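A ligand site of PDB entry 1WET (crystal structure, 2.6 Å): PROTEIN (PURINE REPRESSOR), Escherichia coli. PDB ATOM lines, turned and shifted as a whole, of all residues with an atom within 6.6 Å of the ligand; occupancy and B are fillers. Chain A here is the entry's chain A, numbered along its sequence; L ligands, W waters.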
ATOM      1  N   THR A  66       0.291   8.638 -27.569  1.00  0.00           N
ATOM      2  CA  THR A  66      -0.728   7.626 -27.382  1.00  0.00           C
ATOM      3  C   THR A  66      -1.673   8.039 -26.278  1.00  0.00           C
ATOM      4  O   THR A  66      -2.879   8.113 -26.478  1.00  0.00           O
ATOM      5  CB  THR A  66      -0.125   6.306 -27.105  1.00  0.00           C
ATOM      6  OG1 THR A  66       0.575   5.852 -28.280  1.00  0.00           O
ATOM      7  CG2 THR A  66      -1.216   5.323 -26.646  1.00  0.00           C
ATOM      8  N   SER A  67      -1.129   8.355 -25.114  1.00  0.00           N
ATOM      9  CA  SER A  67      -1.938   8.790 -23.988  1.00  0.00           C
ATOM     10  C   SER A  67      -0.949   9.561 -23.098  1.00  0.00           C
ATOM     11  O   SER A  67       0.254   9.477 -23.284  1.00  0.00           O
ATOM     12  CB  SER A  67      -2.630   7.566 -23.306  1.00  0.00           C
ATOM     13  OG  SER A  67      -2.145   7.284 -21.999  1.00  0.00           O
ATOM     14  N   ALA A  70      -0.640   7.931 -18.185  1.00  0.00           N
ATOM     15  CA  ALA A  70       0.295   6.823 -18.082  1.00  0.00           C
ATOM     16  C   ALA A  70       1.689   7.344 -17.743  1.00  0.00           C
ATOM     17  O   ALA A  70       2.438   8.028 -18.495  1.00  0.00           O
ATOM     18  CB  ALA A  70       0.341   6.007 -19.365  1.00  0.00           C
ATOM     19  N   ALA A  71       1.973   7.040 -16.493  1.00  0.00           N
ATOM     20  CA  ALA A  71       3.222   7.393 -15.809  1.00  0.00           C
ATOM     21  C   ALA A  71       4.424   7.412 -16.709  1.00  0.00           C
ATOM     22  O   ALA A  71       5.148   8.408 -16.831  1.00  0.00           O
ATOM     23  CB  ALA A  71       3.524   6.410 -14.630  1.00  0.00           C
ATOM     24  N   TYR A  72       4.651   6.260 -17.326  1.00  0.00           N
ATOM     25  CA  TYR A  72       5.786   6.061 -18.254  1.00  0.00           C
ATOM     26  C   TYR A  72       5.777   7.261 -19.236  1.00  0.00           C
ATOM     27  O   TYR A  72       6.641   8.137 -19.236  1.00  0.00           O
ATOM     28  CB  TYR A  72       5.536   4.774 -19.047  1.00  0.00           C
ATOM     29  CG  TYR A  72       6.555   4.460 -20.095  1.00  0.00           C
ATOM     30  CD1 TYR A  72       7.806   4.002 -19.758  1.00  0.00           C
ATOM     31  CD2 TYR A  72       6.262   4.617 -21.421  1.00  0.00           C
ATOM     32  CE1 TYR A  72       8.776   3.730 -20.752  1.00  0.00           C
ATOM     33  CE2 TYR A  72       7.199   4.325 -22.416  1.00  0.00           C
ATOM     34  CZ  TYR A  72       8.454   3.896 -22.068  1.00  0.00           C
ATOM     35  OH  TYR A  72       9.355   3.642 -23.053  1.00  0.00           O
ATOM     36  N   PHE A  73       4.705   7.305 -19.996  1.00  0.00           N
ATOM     37  CA  PHE A  73       4.475   8.348 -20.967  1.00  0.00           C
ATOM     38  C   PHE A  73       4.694   9.711 -20.439  1.00  0.00           C
ATOM     39  O   PHE A  73       5.482  10.508 -20.960  1.00  0.00           O
ATOM     40  CB  PHE A  73       3.035   8.270 -21.404  1.00  0.00           C
ATOM     41  CG  PHE A  73       2.773   7.121 -22.274  1.00  0.00           C
ATOM     42  CD1 PHE A  73       3.797   6.611 -23.055  1.00  0.00           C
ATOM     43  CD2 PHE A  73       1.536   6.525 -22.317  1.00  0.00           C
ATOM     44  CE1 PHE A  73       3.589   5.520 -23.850  1.00  0.00           C
ATOM     45  CE2 PHE A  73       1.303   5.448 -23.152  1.00  0.00           C
ATOM     46  CZ  PHE A  73       2.351   4.917 -23.899  1.00  0.00           C
ATOM     47  N   SER A 123       2.988   3.905 -30.146  1.00  0.00           N
ATOM     48  CA  SER A 123       2.830   2.559 -29.575  1.00  0.00           C
ATOM     49  C   SER A 123       2.653   1.482 -30.591  1.00  0.00           C
ATOM     50  O   SER A 123       3.519   0.665 -30.759  1.00  0.00           O
ATOM     51  CB  SER A 123       1.717   2.489 -28.514  1.00  0.00           C
ATOM     52  OG  SER A 123       1.910   3.426 -27.464  1.00  0.00           O
ATOM     53  N   PRO A 186       1.401  -5.759 -24.087  1.00  0.00           N
ATOM     54  CA  PRO A 186       0.900  -5.919 -25.453  1.00  0.00           C
ATOM     55  C   PRO A 186       1.969  -6.205 -26.452  1.00  0.00           C
ATOM     56  O   PRO A 186       2.879  -5.416 -26.668  1.00  0.00           O
ATOM     57  CB  PRO A 186       0.274  -4.551 -25.778  1.00  0.00           C
ATOM     58  CG  PRO A 186       0.366  -3.737 -24.522  1.00  0.00           C
ATOM     59  CD  PRO A 186       1.507  -4.337 -23.740  1.00  0.00           C
ATOM     60  N   ARG A 189       3.491  -4.004 -29.338  1.00  0.00           N
ATOM     61  CA  ARG A 189       4.337  -2.908 -28.911  1.00  0.00           C
ATOM     62  C   ARG A 189       5.740  -3.444 -28.685  1.00  0.00           C
ATOM     63  O   ARG A 189       5.941  -4.632 -28.445  1.00  0.00           O
ATOM     64  CB  ARG A 189       3.825  -2.265 -27.624  1.00  0.00           C
ATOM     65  CG  ARG A 189       2.745  -1.295 -27.907  1.00  0.00           C
ATOM     66  CD  ARG A 189       1.623  -1.509 -27.000  1.00  0.00           C
ATOM     67  NE  ARG A 189       1.583  -0.457 -26.003  1.00  0.00           N
ATOM     68  CZ  ARG A 189       0.522   0.287 -25.817  1.00  0.00           C
ATOM     69  NH1 ARG A 189      -0.538   0.053 -26.584  1.00  0.00           N
ATOM     70  NH2 ARG A 189       0.497   1.263 -24.903  1.00  0.00           N
ATOM     71  N   THR A 191       8.195  -2.353 -26.325  1.00  0.00           N
ATOM     72  CA  THR A 191       8.388  -2.434 -24.881  1.00  0.00           C
ATOM     73  C   THR A 191       7.563  -3.652 -24.438  1.00  0.00           C
ATOM     74  O   THR A 191       7.695  -4.074 -23.281  1.00  0.00           O
ATOM     75  CB  THR A 191       7.670  -1.249 -24.168  1.00  0.00           C
ATOM     76  OG1 THR A 191       6.352  -1.141 -24.689  1.00  0.00           O
ATOM     77  CG2 THR A 191       8.404   0.128 -24.314  1.00  0.00           C
ATOM     78  N   GLY A 192       6.697  -4.161 -25.360  1.00  0.00           N
ATOM     79  CA  GLY A 192       5.830  -5.323 -25.172  1.00  0.00           C
ATOM     80  C   GLY A 192       6.631  -6.566 -25.621  1.00  0.00           C
ATOM     81  O   GLY A 192       7.243  -7.257 -24.824  1.00  0.00           O
ATOM     82  N   ARG A 195      10.605  -6.786 -24.931  1.00  0.00           N
ATOM     83  CA  ARG A 195      11.170  -7.074 -23.635  1.00  0.00           C
ATOM     84  C   ARG A 195      10.996  -8.550 -23.341  1.00  0.00           C
ATOM     85  O   ARG A 195      11.823  -9.191 -22.691  1.00  0.00           O
ATOM     86  CB  ARG A 195      10.489  -6.209 -22.580  1.00  0.00           C
ATOM     87  CG  ARG A 195      10.787  -4.709 -22.715  1.00  0.00           C
ATOM     88  CD  ARG A 195       9.983  -3.846 -21.678  1.00  0.00           C
ATOM     89  NE  ARG A 195      10.310  -2.405 -21.720  1.00  0.00           N
ATOM     90  CZ  ARG A 195       9.625  -1.448 -21.106  1.00  0.00           C
ATOM     91  NH1 ARG A 195       8.563  -1.762 -20.374  1.00  0.00           N
ATOM     92  NH2 ARG A 195       9.975  -0.161 -21.207  1.00  0.00           N
ATOM     93  N   ASP A 219      -1.450  -5.102 -20.248  1.00  0.00           N
ATOM     94  CA  ASP A 219      -1.706  -3.996 -21.147  1.00  0.00           C
ATOM     95  C   ASP A 219      -1.071  -2.709 -20.573  1.00  0.00           C
ATOM     96  O   ASP A 219      -1.437  -1.600 -20.950  1.00  0.00           O
ATOM     97  CB  ASP A 219      -3.238  -3.875 -21.318  1.00  0.00           C
ATOM     98  CG  ASP A 219      -3.964  -3.440 -20.024  1.00  0.00           C
ATOM     99  OD1 ASP A 219      -3.315  -3.096 -18.991  1.00  0.00           O
ATOM    100  OD2 ASP A 219      -5.210  -3.423 -20.043  1.00  0.00           O
ATOM    101  N   PHE A 220      -0.161  -2.894 -19.604  1.00  0.00           N
ATOM    102  CA  PHE A 220       0.602  -1.825 -18.885  1.00  0.00           C
ATOM    103  C   PHE A 220      -0.151  -1.082 -17.784  1.00  0.00           C
ATOM    104  O   PHE A 220       0.406  -0.276 -17.043  1.00  0.00           O
ATOM    105  CB  PHE A 220       1.170  -0.790 -19.861  1.00  0.00           C
ATOM    106  CG  PHE A 220       2.334  -1.281 -20.662  1.00  0.00           C
ATOM    107  CD1 PHE A 220       3.493  -1.681 -20.065  1.00  0.00           C
ATOM    108  CD2 PHE A 220       2.239  -1.373 -22.052  1.00  0.00           C
ATOM    109  CE1 PHE A 220       4.568  -2.134 -20.799  1.00  0.00           C
ATOM    110  CE2 PHE A 220       3.282  -1.831 -22.788  1.00  0.00           C
ATOM    111  CZ  PHE A 220       4.469  -2.209 -22.147  1.00  0.00           C
ATOM    112  N   GLU A 221      -1.441  -1.326 -17.710  1.00  0.00           N
ATOM    113  CA  GLU A 221      -2.294  -0.683 -16.704  1.00  0.00           C
ATOM    114  C   GLU A 221      -2.379  -1.622 -15.495  1.00  0.00           C
ATOM    115  O   GLU A 221      -2.473  -2.839 -15.620  1.00  0.00           O
ATOM    116  CB  GLU A 221      -3.668  -0.342 -17.296  1.00  0.00           C
ATOM    117  CG  GLU A 221      -3.673   0.788 -18.368  1.00  0.00           C
ATOM    118  CD  GLU A 221      -3.891   2.192 -17.795  1.00  0.00           C
ATOM    119  OE1 GLU A 221      -2.910   2.771 -17.250  1.00  0.00           O
ATOM    120  OE2 GLU A 221      -5.041   2.704 -17.862  1.00  0.00           O
ATOM    121  N   GLY A 245       6.440  -6.916 -17.121  1.00  0.00           N
ATOM    122  CA  GLY A 245       6.715  -6.004 -18.263  1.00  0.00           C
ATOM    123  C   GLY A 245       6.779  -4.509 -18.035  1.00  0.00           C
ATOM    124  O   GLY A 245       7.403  -3.807 -18.828  1.00  0.00           O
ATOM    125  N   GLY A 246       6.136  -4.016 -16.979  1.00  0.00           N
ATOM    126  CA  GLY A 246       6.100  -2.581 -16.648  1.00  0.00           C
ATOM    127  C   GLY A 246       5.899  -2.309 -15.140  1.00  0.00           C
ATOM    128  O   GLY A 246       5.192  -3.048 -14.426  1.00  0.00           O
ATOM    129  N   ASP A 247       6.498  -1.246 -14.655  1.00  0.00           N
ATOM    130  CA  ASP A 247       6.341  -0.991 -13.260  1.00  0.00           C
ATOM    131  C   ASP A 247       4.882  -0.796 -12.780  1.00  0.00           C
ATOM    132  O   ASP A 247       4.468  -1.330 -11.719  1.00  0.00           O
ATOM    133  CB  ASP A 247       7.150   0.232 -12.864  1.00  0.00           C
ATOM    134  CG  ASP A 247       8.618  -0.005 -12.886  1.00  0.00           C
ATOM    135  OD1 ASP A 247       9.034  -1.152 -13.165  1.00  0.00           O
ATOM    136  OD2 ASP A 247       9.383   0.965 -12.620  1.00  0.00           O
ATOM    137  N   ILE A 248       4.100  -0.029 -13.522  1.00  0.00           N
ATOM    138  CA  ILE A 248       2.719   0.223 -13.091  1.00  0.00           C
ATOM    139  C   ILE A 248       1.942  -1.087 -12.922  1.00  0.00           C
ATOM    140  O   ILE A 248       1.233  -1.305 -11.944  1.00  0.00           O
ATOM    141  CB  ILE A 248       2.019   1.223 -14.008  1.00  0.00           C
ATOM    142  CG1 ILE A 248       2.744   2.597 -13.995  1.00  0.00           C
ATOM    143  CG2 ILE A 248       0.553   1.356 -13.623  1.00  0.00           C
ATOM    144  CD1 ILE A 248       2.601   3.374 -12.739  1.00  0.00           C
ATOM    145  N   TYR A 273       9.892  -3.266 -14.639  1.00  0.00           N
ATOM    146  CA  TYR A 273      10.562  -2.715 -15.759  1.00  0.00           C
ATOM    147  C   TYR A 273       9.986  -1.398 -16.067  1.00  0.00           C
ATOM    148  O   TYR A 273       8.782  -1.339 -16.388  1.00  0.00           O
ATOM    149  CB  TYR A 273      10.280  -3.566 -16.979  1.00  0.00           C
ATOM    150  CG  TYR A 273      11.274  -3.277 -18.051  1.00  0.00           C
ATOM    151  CD1 TYR A 273      11.599  -1.984 -18.414  1.00  0.00           C
ATOM    152  CD2 TYR A 273      11.950  -4.313 -18.695  1.00  0.00           C
ATOM    153  CE1 TYR A 273      12.536  -1.720 -19.369  1.00  0.00           C
ATOM    154  CE2 TYR A 273      12.902  -4.066 -19.680  1.00  0.00           C
ATOM    155  CZ  TYR A 273      13.192  -2.749 -20.018  1.00  0.00           C
ATOM    156  OH  TYR A 273      14.140  -2.430 -20.992  1.00  0.00           O
ATOM    157  N   ASP A 274      10.888  -0.417 -16.057  1.00  0.00           N
ATOM    158  CA  ASP A 274      10.664   0.984 -16.413  1.00  0.00           C
ATOM    159  C   ASP A 274      11.371   1.953 -15.538  1.00  0.00           C
ATOM    160  O   ASP A 274      11.890   2.975 -15.983  1.00  0.00           O
ATOM    161  CB  ASP A 274       9.201   1.357 -16.486  1.00  0.00           C
ATOM    162  CG  ASP A 274       8.571   1.006 -17.822  1.00  0.00           C
ATOM    163  OD1 ASP A 274       9.251   0.443 -18.729  1.00  0.00           O
ATOM    164  OD2 ASP A 274       7.347   1.208 -17.918  1.00  0.00           O
ATOM    165  N   GLN A 291      14.682   2.605 -17.507  1.00  0.00           N
ATOM    166  CA  GLN A 291      14.634   3.114 -18.902  1.00  0.00           C
ATOM    167  C   GLN A 291      14.936   4.598 -18.850  1.00  0.00           C
ATOM    168  O   GLN A 291      14.305   5.347 -18.118  1.00  0.00           O
ATOM    169  CB  GLN A 291      13.255   2.957 -19.522  1.00  0.00           C
ATOM    170  CG  GLN A 291      13.187   3.623 -20.909  1.00  0.00           C
ATOM    171  CD  GLN A 291      13.218   2.624 -22.072  1.00  0.00           C
ATOM    172  OE1 GLN A 291      12.334   2.625 -22.913  1.00  0.00           O
ATOM    173  NE2 GLN A 291      14.240   1.757 -22.110  1.00  0.00           N
HETATM  174  N1  LIG L   1       6.072   1.212 -20.579  1.00  0.00           N
HETATM  175  C1  LIG L   1       6.612   0.732 -21.736  1.00  0.00           C
HETATM  176  N2  LIG L   1       5.766   0.762 -22.756  1.00  0.00           N
HETATM  177  C2  LIG L   1       4.610   1.285 -22.208  1.00  0.00           C
HETATM  178  C3  LIG L   1       3.359   1.554 -22.820  1.00  0.00           C
HETATM  179  O1  LIG L   1       2.991   1.349 -24.008  1.00  0.00           O
HETATM  180  N3  LIG L   1       2.467   2.095 -21.902  1.00  0.00           N
HETATM  181  C4  LIG L   1       2.714   2.323 -20.577  1.00  0.00           C
HETATM  182  N4  LIG L   1       1.734   2.890 -19.870  1.00  0.00           N
HETATM  183  N5  LIG L   1       3.879   2.077 -20.005  1.00  0.00           N
HETATM  184  C5  LIG L   1       4.781   1.568 -20.868  1.00  0.00           C
HETATM  185  O   HOH W   1       0.517   2.749 -17.252  1.00  0.00           O
HETATM  186  O   HOH W   2      -0.688   1.945 -22.573  1.00  0.00           O
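OE1 of Gln 291 sits at hydrogen-bond distance from OH of Tyr 72 (3.2 Å). O of Gly 245 sits at hydrogen-bond distance from NH1 of Arg 195 (2.8 Å). The backbone carbonyl oxygen of Asp 274 is in hydrogen-bond range of the backbone NH of Gln 291, 3.2 Å away. The side-chain carboxylate (OD1) of Asp 274 lies within salt-bridge range of the guanidinium group (NH2) of Arg 195 (2.7 Å). O of Thr 191 sits close to NE of Arg 195, at 3.5 Å.
N1 of the ligand is in hydrogen-bond range of OD2 of Asp 274, at 3.0 Å. An oxygen (O1) of the ligand is in hydrogen-bond range of the guanidinium group (NH2) of Arg 189. A nitrogen (N2) of the ligand lies within hydrogen-bond range of the side-chain hydroxyl of Thr 191, 2.8 Å away.
Ala 70 touches the ligand. Tyr 72 touches the ligand (CB to N5, 3.3 Å). Phe 73 touches the ligand (CZ to N3, 3.5 Å). Arg 195 touches the ligand. Phe 220 touches the ligand (CD2 to C3, 3.2 Å). Hydrophobic or aromatic side chains that line the ligand: Ala 70, Tyr 72, Phe 73 and Phe 220. The nearest printed residue that does not touch the ligand is Ser 123 (4.2 Å).
Water W1 lies within hydrogen-bond range of a nitrogen (N4) of the ligand, the backbone carbonyl oxygen of Phe 220 and the side-chain carboxylate of Glu 221. Water W2 bridges the guanidinium group of Arg 189 (2.7 Å) and a nitrogen (N3) of the ligand (3.2 Å).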
